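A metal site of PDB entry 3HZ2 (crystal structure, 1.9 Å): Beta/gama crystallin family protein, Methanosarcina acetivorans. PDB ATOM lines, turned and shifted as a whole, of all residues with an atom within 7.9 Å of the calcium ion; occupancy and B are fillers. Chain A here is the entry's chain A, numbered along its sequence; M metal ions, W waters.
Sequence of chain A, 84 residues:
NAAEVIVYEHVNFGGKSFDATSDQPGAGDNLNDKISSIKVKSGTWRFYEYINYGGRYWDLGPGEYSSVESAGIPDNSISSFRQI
N of Glu 49 sits at hydrogen-bond distance from O of Gly 54. N of Ser 79 is in hydrogen-bond range of O of Tyr 48. OG of Ser 77 is in hydrogen-bond range of O of Pro 74, 2.6 Å away. N of Asp 33 is in hydrogen-bond range of O of Ile 78, 2.9 Å away. OG of Ser 79 sits close to OD1 of Asn 32 (2.5 Å).
The nearest printed residue that does not touch the calcium ion is Ile 78 (4.3 Å).
The calcium ion is bound by the backbone carbonyl oxygen (O) of Glu 49 (2.4 Å), the side-chain carboxylate (OD1) of Asp 33 (2.5 Å), the backbone carbonyl oxygen (O) of Ser 77 (2.5 Å), the side-chain hydroxyl (OG) of Ser 79 (2.6 Å), water W2 (2.8 Å) and water W1 (2.8 Å). The calcium ion has six donor atoms within binding distance.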
ATOM      1  N   ASN A  32      -9.550  22.806  -1.588  1.00  0.00           N
ATOM      2  CA  ASN A  32      -9.991  22.336  -2.891  1.00  0.00           C
ATOM      3  C   ASN A  32      -9.121  21.142  -3.316  1.00  0.00           C
ATOM      4  O   ASN A  32      -7.895  21.207  -3.264  1.00  0.00           O
ATOM      5  CB  ASN A  32      -9.896  23.451  -3.929  1.00  0.00           C
ATOM      6  CG  ASN A  32     -10.268  22.993  -5.316  1.00  0.00           C
ATOM      7  OD1 ASN A  32     -11.093  22.092  -5.476  1.00  0.00           O
ATOM      8  ND2 ASN A  32      -9.674  23.602  -6.327  1.00  0.00           N
ATOM      9  N   ASP A  33      -9.779  20.062  -3.712  1.00  0.00           N
ATOM     10  CA  ASP A  33      -9.085  18.846  -4.124  1.00  0.00           C
ATOM     11  C   ASP A  33      -8.228  18.238  -3.028  1.00  0.00           C
ATOM     12  O   ASP A  33      -7.154  17.691  -3.317  1.00  0.00           O
ATOM     13  CB  ASP A  33      -8.242  19.114  -5.365  1.00  0.00           C
ATOM     14  CG  ASP A  33      -9.090  19.359  -6.583  1.00  0.00           C
ATOM     15  OD1 ASP A  33     -10.205  18.814  -6.578  1.00  0.00           O
ATOM     16  OD2 ASP A  33      -8.657  20.059  -7.509  1.00  0.00           O
ATOM     17  N   LYS A  34      -8.695  18.314  -1.788  1.00  0.00           N
ATOM     18  CA  LYS A  34      -7.971  17.764  -0.655  1.00  0.00           C
ATOM     19  C   LYS A  34      -8.859  17.024   0.356  1.00  0.00           C
ATOM     20  O   LYS A  34      -8.365  16.216   1.123  1.00  0.00           O
ATOM     21  CB  LYS A  34      -7.241  18.861   0.120  1.00  0.00           C
ATOM     22  CG  LYS A  34      -6.232  19.674  -0.657  1.00  0.00           C
ATOM     23  CD  LYS A  34      -5.546  20.642   0.294  1.00  0.00           C
ATOM     24  CE  LYS A  34      -4.695  21.655  -0.418  1.00  0.00           C
ATOM     25  NZ  LYS A  34      -4.101  22.600   0.564  1.00  0.00           N
ATOM     26  N   TYR A  48     -19.687  18.760  -4.803  1.00  0.00           N
ATOM     27  CA  TYR A  48     -19.433  18.738  -6.245  1.00  0.00           C
ATOM     28  C   TYR A  48     -17.970  18.506  -6.573  1.00  0.00           C
ATOM     29  O   TYR A  48     -17.092  18.900  -5.809  1.00  0.00           O
ATOM     30  CB  TYR A  48     -19.860  20.066  -6.861  1.00  0.00           C
ATOM     31  CG  TYR A  48     -21.354  20.251  -6.999  1.00  0.00           C
ATOM     32  CD1 TYR A  48     -22.031  19.825  -8.145  1.00  0.00           C
ATOM     33  CD2 TYR A  48     -22.092  20.880  -5.992  1.00  0.00           C
ATOM     34  CE1 TYR A  48     -23.401  20.024  -8.291  1.00  0.00           C
ATOM     35  CE2 TYR A  48     -23.466  21.089  -6.138  1.00  0.00           C
ATOM     36  CZ  TYR A  48     -24.108  20.654  -7.281  1.00  0.00           C
ATOM     37  OH  TYR A  48     -25.466  20.879  -7.425  1.00  0.00           O
ATOM     38  N   GLU A  49     -17.712  17.875  -7.708  1.00  0.00           N
ATOM     39  CA  GLU A  49     -16.330  17.612  -8.074  1.00  0.00           C
ATOM     40  C   GLU A  49     -15.639  18.824  -8.689  1.00  0.00           C
ATOM     41  O   GLU A  49     -14.440  18.841  -8.821  1.00  0.00           O
ATOM     42  CB  GLU A  49     -16.242  16.410  -9.010  1.00  0.00           C
ATOM     43  CG  GLU A  49     -16.705  16.654 -10.421  1.00  0.00           C
ATOM     44  CD  GLU A  49     -16.613  15.392 -11.276  1.00  0.00           C
ATOM     45  OE1 GLU A  49     -15.535  14.749 -11.263  1.00  0.00           O
ATOM     46  OE2 GLU A  49     -17.602  15.066 -11.950  1.00  0.00           O
ATOM     47  N   TYR A  50     -16.386  19.857  -9.078  1.00  0.00           N
ATOM     48  CA  TYR A  50     -15.746  21.029  -9.678  1.00  0.00           C
ATOM     49  C   TYR A  50     -16.146  22.280  -8.914  1.00  0.00           C
ATOM     50  O   TYR A  50     -17.186  22.295  -8.254  1.00  0.00           O
ATOM     51  CB  TYR A  50     -16.170  21.158 -11.147  1.00  0.00           C
ATOM     52  CG  TYR A  50     -15.718  19.998 -12.015  1.00  0.00           C
ATOM     53  CD1 TYR A  50     -16.460  19.624 -13.137  1.00  0.00           C
ATOM     54  CD2 TYR A  50     -14.564  19.275 -11.714  1.00  0.00           C
ATOM     55  CE1 TYR A  50     -16.060  18.553 -13.940  1.00  0.00           C
ATOM     56  CE2 TYR A  50     -14.154  18.208 -12.516  1.00  0.00           C
ATOM     57  CZ  TYR A  50     -14.905  17.852 -13.619  1.00  0.00           C
ATOM     58  OH  TYR A  50     -14.520  16.787 -14.402  1.00  0.00           O
ATOM     59  N   ILE A  51     -15.331  23.330  -8.996  1.00  0.00           N
ATOM     60  CA  ILE A  51     -15.673  24.558  -8.287  1.00  0.00           C
ATOM     61  C   ILE A  51     -16.978  25.100  -8.865  1.00  0.00           C
ATOM     62  O   ILE A  51     -17.407  24.683  -9.947  1.00  0.00           O
ATOM     63  CB  ILE A  51     -14.576  25.638  -8.400  1.00  0.00           C
ATOM     64  CG1 ILE A  51     -14.384  26.040  -9.865  1.00  0.00           C
ATOM     65  CG2 ILE A  51     -13.269  25.140  -7.811  1.00  0.00           C
ATOM     66  CD1 ILE A  51     -13.502  27.251 -10.039  1.00  0.00           C
ATOM     67  N   GLY A  54     -19.866  22.445 -10.089  1.00  0.00           N
ATOM     68  CA  GLY A  54     -19.818  21.816 -11.386  1.00  0.00           C
ATOM     69  C   GLY A  54     -19.514  20.331 -11.296  1.00  0.00           C
ATOM     70  O   GLY A  54     -19.002  19.836 -10.284  1.00  0.00           O
ATOM     71  N   TRP A  58     -22.531  14.438  -4.840  1.00  0.00           N
ATOM     72  CA  TRP A  58     -22.916  13.426  -3.861  1.00  0.00           C
ATOM     73  C   TRP A  58     -23.593  14.137  -2.697  1.00  0.00           C
ATOM     74  O   TRP A  58     -23.080  15.144  -2.196  1.00  0.00           O
ATOM     75  CB  TRP A  58     -21.677  12.686  -3.381  1.00  0.00           C
ATOM     76  CG  TRP A  58     -20.943  11.978  -4.479  1.00  0.00           C
ATOM     77  CD1 TRP A  58     -21.149  10.712  -4.931  1.00  0.00           C
ATOM     78  CD2 TRP A  58     -19.906  12.533  -5.316  1.00  0.00           C
ATOM     79  NE1 TRP A  58     -20.320  10.425  -5.986  1.00  0.00           N
ATOM     80  CE2 TRP A  58     -19.550  11.528  -6.243  1.00  0.00           C
ATOM     81  CE3 TRP A  58     -19.260  13.766  -5.372  1.00  0.00           C
ATOM     82  CZ2 TRP A  58     -18.560  11.730  -7.217  1.00  0.00           C
ATOM     83  CZ3 TRP A  58     -18.280  13.965  -6.338  1.00  0.00           C
ATOM     84  CH2 TRP A  58     -17.940  12.943  -7.256  1.00  0.00           C
ATOM     85  N   PRO A  74     -14.793  10.225  -4.611  1.00  0.00           N
ATOM     86  CA  PRO A  74     -13.369   9.960  -4.853  1.00  0.00           C
ATOM     87  C   PRO A  74     -12.520  10.849  -3.947  1.00  0.00           C
ATOM     88  O   PRO A  74     -12.883  11.993  -3.673  1.00  0.00           O
ATOM     89  CB  PRO A  74     -13.200  10.289  -6.341  1.00  0.00           C
ATOM     90  CG  PRO A  74     -14.302  11.290  -6.604  1.00  0.00           C
ATOM     91  CD  PRO A  74     -15.460  10.730  -5.820  1.00  0.00           C
ATOM     92  N   ASP A  75     -11.402  10.320  -3.477  1.00  0.00           N
ATOM     93  CA  ASP A  75     -10.539  11.086  -2.571  1.00  0.00           C
ATOM     94  C   ASP A  75      -9.891  12.290  -3.261  1.00  0.00           C
ATOM     95  O   ASP A  75      -9.580  12.243  -4.446  1.00  0.00           O
ATOM     96  CB  ASP A  75      -9.467  10.159  -1.979  1.00  0.00           C
ATOM     97  CG  ASP A  75      -8.732  10.799  -0.825  1.00  0.00           C
ATOM     98  OD1 ASP A  75      -9.374  11.553  -0.059  1.00  0.00           O
ATOM     99  OD2 ASP A  75      -7.523  10.540  -0.666  1.00  0.00           O
ATOM    100  N   ASN A  76      -9.699  13.367  -2.500  1.00  0.00           N
ATOM    101  CA  ASN A  76      -9.077  14.589  -3.011  1.00  0.00           C
ATOM    102  C   ASN A  76      -9.743  15.135  -4.269  1.00  0.00           C
ATOM    103  O   ASN A  76      -9.057  15.611  -5.172  1.00  0.00           O
ATOM    104  CB  ASN A  76      -7.599  14.342  -3.317  1.00  0.00           C
ATOM    105  CG  ASN A  76      -6.836  13.894  -2.099  1.00  0.00           C
ATOM    106  OD1 ASN A  76      -7.266  14.162  -0.994  1.00  0.00           O
ATOM    107  ND2 ASN A  76      -5.692  13.248  -2.301  1.00  0.00           N
ATOM    108  N   SER A  77     -11.059  15.080  -4.321  1.00  0.00           N
ATOM    109  CA  SER A  77     -11.754  15.543  -5.522  1.00  0.00           C
ATOM    110  C   SER A  77     -12.840  16.596  -5.301  1.00  0.00           C
ATOM    111  O   SER A  77     -13.285  17.213  -6.256  1.00  0.00           O
ATOM    112  CB  SER A  77     -12.369  14.351  -6.246  1.00  0.00           C
ATOM    113  OG  SER A  77     -13.406  13.784  -5.460  1.00  0.00           O
ATOM    114  N   ILE A  78     -13.276  16.790  -4.067  1.00  0.00           N
ATOM    115  CA  ILE A  78     -14.324  17.794  -3.822  1.00  0.00           C
ATOM    116  C   ILE A  78     -13.777  19.186  -4.119  1.00  0.00           C
ATOM    117  O   ILE A  78     -12.674  19.536  -3.704  1.00  0.00           O
ATOM    118  CB  ILE A  78     -14.820  17.715  -2.365  1.00  0.00           C
ATOM    119  CG1 ILE A  78     -15.538  16.374  -2.156  1.00  0.00           C
ATOM    120  CG2 ILE A  78     -15.746  18.894  -2.067  1.00  0.00           C
ATOM    121  CD1 ILE A  78     -15.927  16.101  -0.719  1.00  0.00           C
ATOM    122  N   SER A  79     -14.565  19.991  -4.834  1.00  0.00           N
ATOM    123  CA  SER A  79     -14.139  21.347  -5.173  1.00  0.00           C
ATOM    124  C   SER A  79     -15.144  22.425  -4.783  1.00  0.00           C
ATOM    125  O   SER A  79     -14.862  23.616  -4.896  1.00  0.00           O
ATOM    126  CB  SER A  79     -13.826  21.463  -6.659  1.00  0.00           C
ATOM    127  OG  SER A  79     -12.618  20.785  -6.945  1.00  0.00           O
ATOM    128  N   SER A  80     -16.310  22.002  -4.320  1.00  0.00           N
ATOM    129  CA  SER A  80     -17.340  22.933  -3.873  1.00  0.00           C
ATOM    130  C   SER A  80     -18.456  22.151  -3.207  1.00  0.00           C
ATOM    131  O   SER A  80     -18.629  20.969  -3.454  1.00  0.00           O
ATOM    132  CB  SER A  80     -17.905  23.755  -5.049  1.00  0.00           C
ATOM    133  OG  SER A  80     -18.551  22.941  -6.014  1.00  0.00           O
HETATM  134 CA    CA M   1     -12.142  18.494  -8.081  1.00  0.00          CA
HETATM  135  O   HOH W   1     -11.158  20.181 -10.050  1.00  0.00           O
HETATM  136  O   HOH W   2     -10.803  16.375  -9.260  1.00  0.00           O
